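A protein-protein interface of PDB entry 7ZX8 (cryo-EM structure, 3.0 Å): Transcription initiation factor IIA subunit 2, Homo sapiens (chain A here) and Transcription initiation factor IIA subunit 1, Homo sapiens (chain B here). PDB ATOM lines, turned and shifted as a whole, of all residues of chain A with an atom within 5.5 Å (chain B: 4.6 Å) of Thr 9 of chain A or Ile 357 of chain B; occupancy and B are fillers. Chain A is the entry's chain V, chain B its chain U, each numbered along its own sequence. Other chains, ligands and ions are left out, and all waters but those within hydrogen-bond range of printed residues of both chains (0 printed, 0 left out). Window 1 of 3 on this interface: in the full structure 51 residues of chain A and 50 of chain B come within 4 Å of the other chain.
OD1 of Asn 13 of chain A sits close to O of Thr 9 of chain A (3.1 Å). The side-chain hydroxyl of Thr 9 of chain A lies close to the backbone NH of Leu 11 of chain A, 3.4 Å away. N of Val 336 of chain B sits at hydrogen-bond distance from O of Ile 357 of chain B (2.9 Å). O of Leu 11 of chain A is in hydrogen-bond range of OG of Ser 14 of chain A (2.5 Å). The backbone NH (N) of Gly 356 of chain B lies within hydrogen-bond range of the backbone carbonyl oxygen (O) of Phe 367 of chain B, at 2.9 Å.
Hydrophobic or aromatic side chains of chain A within 4 Å of the printed part of chain B: Tyr 6, Leu 11 and Leu 48. Of the 11 printed residues of chain B, 5 touch a printed residue of chain A. Hydrophobic or aromatic side chains of chain B within 4 Å of the printed part of chain A: Tyr 14, Val 336, Ile 357 and Ile 366. Along chain B the printed residues that touch a printed residue of chain A span positions 14 to 366. Among the printed residues, 6 pairs touch across the chains. Among the printed residues, no Asp or Glu carboxylate lies within 4 Å of a Lys or Arg side-chain nitrogen of the other chain.
Of chain B, only Ile 357 comes within 4 Å of Thr 9 of chain A. Ile 357 of chain B touches just these residues of chain A: Thr 9 and Leu 48. Of the printed residues of chain A, Tyr 14 of chain B touches Leu 11 (3.7 Å). Printed residues of chain A within 4 Å of Ile 366 of chain B: Leu 48 (3.9 Å). Of the printed residues of chain A, Gly 356 of chain B touches Leu 48. Phe 367 of chain B touches none of the printed residues of chain A. Ile 44 of chain A touches none of the printed residues of chain B. The nearest residue of chain A that does not touch Ile 357 of chain B is Ile 44 of chain A (4.3 Å).
CE1 of Tyr 6 of chain A touches O of Val 336 of chain B, 3.6 Å away. Thr 9 of chain A touches Ile 357 of chain B (CG2 to CG2, 3.9 Å). Leu 11 of chain A touches Tyr 14 of chain B (CD2 to CD2, 3.7 Å). CD2 of Leu 48 of chain A touches N of Gly 356 of chain B, at 3.2 Å. CD1 of Ile 357 of chain B touches CD1 of Leu 48 of chain A, at 3.3 Å. CD1 of Ile 366 of chain B touches CG of Leu 48 of chain A (3.9 Å).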
ATOM      1  N   TYR A   6       3.010  -4.214 -20.845  1.00  0.00           N
ATOM      2  CA  TYR A   6       3.729  -5.148 -19.990  1.00  0.00           C
ATOM      3  C   TYR A   6       5.183  -4.762 -19.761  1.00  0.00           C
ATOM      4  O   TYR A   6       5.890  -5.483 -19.051  1.00  0.00           O
ATOM      5  CB  TYR A   6       3.657  -6.558 -20.584  1.00  0.00           C
ATOM      6  CG  TYR A   6       2.284  -7.181 -20.498  1.00  0.00           C
ATOM      7  CD1 TYR A   6       1.813  -7.707 -19.303  1.00  0.00           C
ATOM      8  CD2 TYR A   6       1.454  -7.241 -21.609  1.00  0.00           C
ATOM      9  CE1 TYR A   6       0.557  -8.277 -19.215  1.00  0.00           C
ATOM     10  CE2 TYR A   6       0.195  -7.808 -21.533  1.00  0.00           C
ATOM     11  CZ  TYR A   6      -0.247  -8.323 -20.333  1.00  0.00           C
ATOM     12  OH  TYR A   6      -1.499  -8.890 -20.250  1.00  0.00           O
ATOM     13  N   ARG A   7       5.650  -3.654 -20.332  1.00  0.00           N
ATOM     14  CA  ARG A   7       6.997  -3.164 -20.040  1.00  0.00           C
ATOM     15  C   ARG A   7       6.982  -2.188 -18.868  1.00  0.00           C
ATOM     16  O   ARG A   7       7.534  -1.091 -18.931  1.00  0.00           O
ATOM     17  CB  ARG A   7       7.605  -2.522 -21.283  1.00  0.00           C
ATOM     18  CG  ARG A   7       6.819  -1.347 -21.845  1.00  0.00           C
ATOM     19  CD  ARG A   7       7.682  -0.517 -22.788  1.00  0.00           C
ATOM     20  NE  ARG A   7       8.197  -1.305 -23.907  1.00  0.00           N
ATOM     21  CZ  ARG A   7       7.595  -1.433 -25.086  1.00  0.00           C
ATOM     22  NH1 ARG A   7       6.440  -0.824 -25.328  1.00  0.00           N
ATOM     23  NH2 ARG A   7       8.151  -2.176 -26.033  1.00  0.00           N
ATOM     24  N   ASN A   8       6.334  -2.601 -17.779  1.00  0.00           N
ATOM     25  CA  ASN A   8       6.304  -1.816 -16.551  1.00  0.00           C
ATOM     26  C   ASN A   8       6.480  -2.651 -15.292  1.00  0.00           C
ATOM     27  O   ASN A   8       6.722  -2.071 -14.230  1.00  0.00           O
ATOM     28  CB  ASN A   8       4.987  -1.035 -16.448  1.00  0.00           C
ATOM     29  CG  ASN A   8       4.913   0.114 -17.434  1.00  0.00           C
ATOM     30  OD1 ASN A   8       5.892   0.831 -17.641  1.00  0.00           O
ATOM     31  ND2 ASN A   8       3.750   0.295 -18.048  1.00  0.00           N
ATOM     32  N   THR A   9       6.369  -3.975 -15.365  1.00  0.00           N
ATOM     33  CA  THR A   9       6.523  -4.818 -14.193  1.00  0.00           C
ATOM     34  C   THR A   9       7.999  -4.932 -13.823  1.00  0.00           C
ATOM     35  O   THR A   9       8.869  -4.254 -14.381  1.00  0.00           O
ATOM     36  CB  THR A   9       5.931  -6.203 -14.451  1.00  0.00           C
ATOM     37  OG1 THR A   9       6.669  -6.855 -15.492  1.00  0.00           O
ATOM     38  CG2 THR A   9       4.476  -6.091 -14.866  1.00  0.00           C
ATOM     39  N   THR A  10       8.287  -5.808 -12.860  1.00  0.00           N
ATOM     40  CA  THR A  10       9.676  -6.073 -12.505  1.00  0.00           C
ATOM     41  C   THR A  10      10.441  -6.635 -13.695  1.00  0.00           C
ATOM     42  O   THR A  10      11.589  -6.249 -13.944  1.00  0.00           O
ATOM     43  CB  THR A  10       9.747  -7.039 -11.320  1.00  0.00           C
ATOM     44  OG1 THR A  10       9.308  -8.340 -11.734  1.00  0.00           O
ATOM     45  CG2 THR A  10       8.877  -6.551 -10.169  1.00  0.00           C
ATOM     46  N   LEU A  11       9.817  -7.542 -14.449  1.00  0.00           N
ATOM     47  CA  LEU A  11      10.481  -8.132 -15.607  1.00  0.00           C
ATOM     48  C   LEU A  11      10.782  -7.074 -16.662  1.00  0.00           C
ATOM     49  O   LEU A  11      11.921  -6.941 -17.122  1.00  0.00           O
ATOM     50  CB  LEU A  11       9.609  -9.248 -16.190  1.00  0.00           C
ATOM     51  CG  LEU A  11      10.238 -10.099 -17.295  1.00  0.00           C
ATOM     52  CD1 LEU A  11      11.552 -10.719 -16.837  1.00  0.00           C
ATOM     53  CD2 LEU A  11       9.268 -11.173 -17.763  1.00  0.00           C
ATOM     54  N   GLY A  12       9.766  -6.302 -17.056  1.00  0.00           N
ATOM     55  CA  GLY A  12       9.976  -5.286 -18.076  1.00  0.00           C
ATOM     56  C   GLY A  12      10.926  -4.196 -17.622  1.00  0.00           C
ATOM     57  O   GLY A  12      11.720  -3.677 -18.414  1.00  0.00           O
ATOM     58  N   ASN A  13      10.852  -3.822 -16.344  1.00  0.00           N
ATOM     59  CA  ASN A  13      11.804  -2.858 -15.808  1.00  0.00           C
ATOM     60  C   ASN A  13      13.223  -3.406 -15.871  1.00  0.00           C
ATOM     61  O   ASN A  13      14.168  -2.668 -16.170  1.00  0.00           O
ATOM     62  CB  ASN A  13      11.427  -2.494 -14.372  1.00  0.00           C
ATOM     63  CG  ASN A  13      10.204  -1.602 -14.302  1.00  0.00           C
ATOM     64  OD1 ASN A  13       9.518  -1.389 -15.302  1.00  0.00           O
ATOM     65  ND2 ASN A  13       9.922  -1.074 -13.117  1.00  0.00           N
ATOM     66  N   SER A  14      13.391  -4.700 -15.592  1.00  0.00           N
ATOM     67  CA  SER A  14      14.703  -5.319 -15.740  1.00  0.00           C
ATOM     68  C   SER A  14      15.168  -5.269 -17.188  1.00  0.00           C
ATOM     69  O   SER A  14      16.343  -5.000 -17.460  1.00  0.00           O
ATOM     70  CB  SER A  14      14.661  -6.765 -15.242  1.00  0.00           C
ATOM     71  OG  SER A  14      14.205  -7.641 -16.259  1.00  0.00           O
ATOM     72  N   ILE A  44       6.107 -11.997 -24.340  1.00  0.00           N
ATOM     73  CA  ILE A  44       5.406 -11.982 -23.062  1.00  0.00           C
ATOM     74  C   ILE A  44       3.902 -12.035 -23.282  1.00  0.00           C
ATOM     75  O   ILE A  44       3.175 -12.660 -22.505  1.00  0.00           O
ATOM     76  CB  ILE A  44       5.822 -10.759 -22.224  1.00  0.00           C
ATOM     77  CG1 ILE A  44       5.284 -10.890 -20.796  1.00  0.00           C
ATOM     78  CG2 ILE A  44       5.324  -9.472 -22.856  1.00  0.00           C
ATOM     79  CD1 ILE A  44       5.898  -9.910 -19.819  1.00  0.00           C
ATOM     80  N   LEU A  48       2.477 -15.232 -21.498  1.00  0.00           N
ATOM     81  CA  LEU A  48       1.642 -14.859 -20.364  1.00  0.00           C
ATOM     82  C   LEU A  48       0.208 -15.337 -20.563  1.00  0.00           C
ATOM     83  O   LEU A  48      -0.470 -15.714 -19.599  1.00  0.00           O
ATOM     84  CB  LEU A  48       1.705 -13.341 -20.181  1.00  0.00           C
ATOM     85  CG  LEU A  48       1.076 -12.655 -18.966  1.00  0.00           C
ATOM     86  CD1 LEU A  48       1.813 -11.354 -18.699  1.00  0.00           C
ATOM     87  CD2 LEU A  48      -0.390 -12.388 -19.160  1.00  0.00           C
ATOM     88  N   TYR B  14       9.212 -16.756 -16.103  1.00  0.00           N
ATOM     89  CA  TYR B  14      10.237 -15.802 -16.505  1.00  0.00           C
ATOM     90  C   TYR B  14      11.372 -16.502 -17.226  1.00  0.00           C
ATOM     91  O   TYR B  14      11.936 -15.957 -18.179  1.00  0.00           O
ATOM     92  CB  TYR B  14      10.742 -15.039 -15.290  1.00  0.00           C
ATOM     93  CG  TYR B  14       9.718 -14.089 -14.735  1.00  0.00           C
ATOM     94  CD1 TYR B  14       9.934 -13.421 -13.550  1.00  0.00           C
ATOM     95  CD2 TYR B  14       8.532 -13.862 -15.404  1.00  0.00           C
ATOM     96  CE1 TYR B  14       8.994 -12.551 -13.044  1.00  0.00           C
ATOM     97  CE2 TYR B  14       7.590 -12.999 -14.907  1.00  0.00           C
ATOM     98  CZ  TYR B  14       7.825 -12.345 -13.728  1.00  0.00           C
ATOM     99  OH  TYR B  14       6.882 -11.480 -13.233  1.00  0.00           O
ATOM    100  N   VAL B 334       0.398  -2.919  -8.495  1.00  0.00           N
ATOM    101  CA  VAL B 334      -0.133  -2.668  -9.829  1.00  0.00           C
ATOM    102  C   VAL B 334      -0.495  -3.999 -10.462  1.00  0.00           C
ATOM    103  O   VAL B 334       0.306  -4.939 -10.439  1.00  0.00           O
ATOM    104  CB  VAL B 334       0.860  -1.902 -10.718  1.00  0.00           C
ATOM    105  CG1 VAL B 334       0.302  -1.749 -12.112  1.00  0.00           C
ATOM    106  CG2 VAL B 334       1.166  -0.535 -10.134  1.00  0.00           C
ATOM    107  N   VAL B 335      -1.699  -4.083 -11.018  1.00  0.00           N
ATOM    108  CA  VAL B 335      -2.126  -5.217 -11.827  1.00  0.00           C
ATOM    109  C   VAL B 335      -2.208  -4.741 -13.267  1.00  0.00           C
ATOM    110  O   VAL B 335      -2.971  -3.820 -13.581  1.00  0.00           O
ATOM    111  CB  VAL B 335      -3.476  -5.779 -11.367  1.00  0.00           C
ATOM    112  CG1 VAL B 335      -3.799  -7.038 -12.134  1.00  0.00           C
ATOM    113  CG2 VAL B 335      -3.456  -6.053  -9.885  1.00  0.00           C
ATOM    114  N   VAL B 336      -1.420  -5.359 -14.134  1.00  0.00           N
ATOM    115  CA  VAL B 336      -1.418  -5.052 -15.556  1.00  0.00           C
ATOM    116  C   VAL B 336      -1.926  -6.281 -16.280  1.00  0.00           C
ATOM    117  O   VAL B 336      -1.290  -7.342 -16.240  1.00  0.00           O
ATOM    118  CB  VAL B 336      -0.021  -4.652 -16.040  1.00  0.00           C
ATOM    119  CG1 VAL B 336       0.024  -4.632 -17.542  1.00  0.00           C
ATOM    120  CG2 VAL B 336       0.350  -3.299 -15.483  1.00  0.00           C
ATOM    121  N   GLY B 356      -2.578 -11.701 -16.885  1.00  0.00           N
ATOM    122  CA  GLY B 356      -2.133 -10.509 -16.190  1.00  0.00           C
ATOM    123  C   GLY B 356      -1.082 -10.735 -15.123  1.00  0.00           C
ATOM    124  O   GLY B 356      -0.903 -11.856 -14.632  1.00  0.00           O
ATOM    125  N   ILE B 357      -0.386  -9.662 -14.757  1.00  0.00           N
ATOM    126  CA  ILE B 357       0.694  -9.704 -13.781  1.00  0.00           C
ATOM    127  C   ILE B 357       0.415  -8.692 -12.683  1.00  0.00           C
ATOM    128  O   ILE B 357       0.008  -7.556 -12.943  1.00  0.00           O
ATOM    129  CB  ILE B 357       2.050  -9.427 -14.450  1.00  0.00           C
ATOM    130  CG1 ILE B 357       2.292 -10.422 -15.573  1.00  0.00           C
ATOM    131  CG2 ILE B 357       3.158  -9.506 -13.438  1.00  0.00           C
ATOM    132  CD1 ILE B 357       3.659 -10.319 -16.180  1.00  0.00           C
ATOM    133  N   MET B 358       0.638  -9.102 -11.444  1.00  0.00           N
ATOM    134  CA  MET B 358       0.349  -8.287 -10.277  1.00  0.00           C
ATOM    135  C   MET B 358       1.609  -8.040  -9.464  1.00  0.00           C
ATOM    136  O   MET B 358       2.576  -8.803  -9.517  1.00  0.00           O
ATOM    137  CB  MET B 358      -0.710  -8.951  -9.399  1.00  0.00           C
ATOM    138  CG  MET B 358      -1.936  -9.390 -10.148  1.00  0.00           C
ATOM    139  SD  MET B 358      -3.076 -10.352  -9.147  1.00  0.00           S
ATOM    140  CE  MET B 358      -2.259 -11.936  -9.136  1.00  0.00           C
ATOM    141  N   ASN B 359       1.574  -6.962  -8.683  1.00  0.00           N
ATOM    142  CA  ASN B 359       2.694  -6.534  -7.854  1.00  0.00           C
ATOM    143  C   ASN B 359       2.224  -6.380  -6.412  1.00  0.00           C
ATOM    144  O   ASN B 359       2.409  -5.346  -5.772  1.00  0.00           O
ATOM    145  CB  ASN B 359       3.302  -5.238  -8.365  1.00  0.00           C
ATOM    146  CG  ASN B 359       4.706  -5.019  -7.857  1.00  0.00           C
ATOM    147  OD1 ASN B 359       5.020  -5.334  -6.711  1.00  0.00           O
ATOM    148  ND2 ASN B 359       5.567  -4.486  -8.713  1.00  0.00           N
ATOM    149  N   TYR B 365       2.864 -11.605  -8.786  1.00  0.00           N
ATOM    150  CA  TYR B 365       2.144 -12.831  -9.077  1.00  0.00           C
ATOM    151  C   TYR B 365       1.680 -12.834 -10.523  1.00  0.00           C
ATOM    152  O   TYR B 365       1.620 -11.793 -11.177  1.00  0.00           O
ATOM    153  CB  TYR B 365       0.941 -12.993  -8.156  1.00  0.00           C
ATOM    154  CG  TYR B 365       1.305 -13.112  -6.706  1.00  0.00           C
ATOM    155  CD1 TYR B 365       1.568 -14.345  -6.138  1.00  0.00           C
ATOM    156  CD2 TYR B 365       1.394 -11.989  -5.902  1.00  0.00           C
ATOM    157  CE1 TYR B 365       1.904 -14.459  -4.811  1.00  0.00           C
ATOM    158  CE2 TYR B 365       1.731 -12.091  -4.575  1.00  0.00           C
ATOM    159  CZ  TYR B 365       1.985 -13.330  -4.034  1.00  0.00           C
ATOM    160  OH  TYR B 365       2.323 -13.439  -2.707  1.00  0.00           O
ATOM    161  N   ILE B 366       1.344 -14.019 -11.013  1.00  0.00           N
ATOM    162  CA  ILE B 366       0.859 -14.208 -12.371  1.00  0.00           C
ATOM    163  C   ILE B 366      -0.550 -14.769 -12.292  1.00  0.00           C
ATOM    164  O   ILE B 366      -0.886 -15.479 -11.340  1.00  0.00           O
ATOM    165  CB  ILE B 366       1.776 -15.153 -13.163  1.00  0.00           C
ATOM    166  CG1 ILE B 366       1.303 -15.248 -14.599  1.00  0.00           C
ATOM    167  CG2 ILE B 366       1.787 -16.529 -12.549  1.00  0.00           C
ATOM    168  CD1 ILE B 366       1.349 -13.936 -15.309  1.00  0.00           C
ATOM    169  N   PHE B 367      -1.384 -14.443 -13.275  1.00  0.00           N
ATOM    170  CA  PHE B 367      -2.669 -15.114 -13.359  1.00  0.00           C
ATOM    171  C   PHE B 367      -3.100 -15.203 -14.808  1.00  0.00           C
ATOM    172  O   PHE B 367      -2.861 -14.280 -15.589  1.00  0.00           O
ATOM    173  CB  PHE B 367      -3.739 -14.409 -12.528  1.00  0.00           C
ATOM    174  CG  PHE B 367      -4.056 -13.026 -12.985  1.00  0.00           C
ATOM    175  CD1 PHE B 367      -4.962 -12.805 -13.994  1.00  0.00           C
ATOM    176  CD2 PHE B 367      -3.472 -11.942 -12.376  1.00  0.00           C
ATOM    177  CE1 PHE B 367      -5.254 -11.529 -14.402  1.00  0.00           C
ATOM    178  CE2 PHE B 367      -3.771 -10.664 -12.784  1.00  0.00           C
ATOM    179  CZ  PHE B 367      -4.661 -10.460 -13.797  1.00  0.00           C
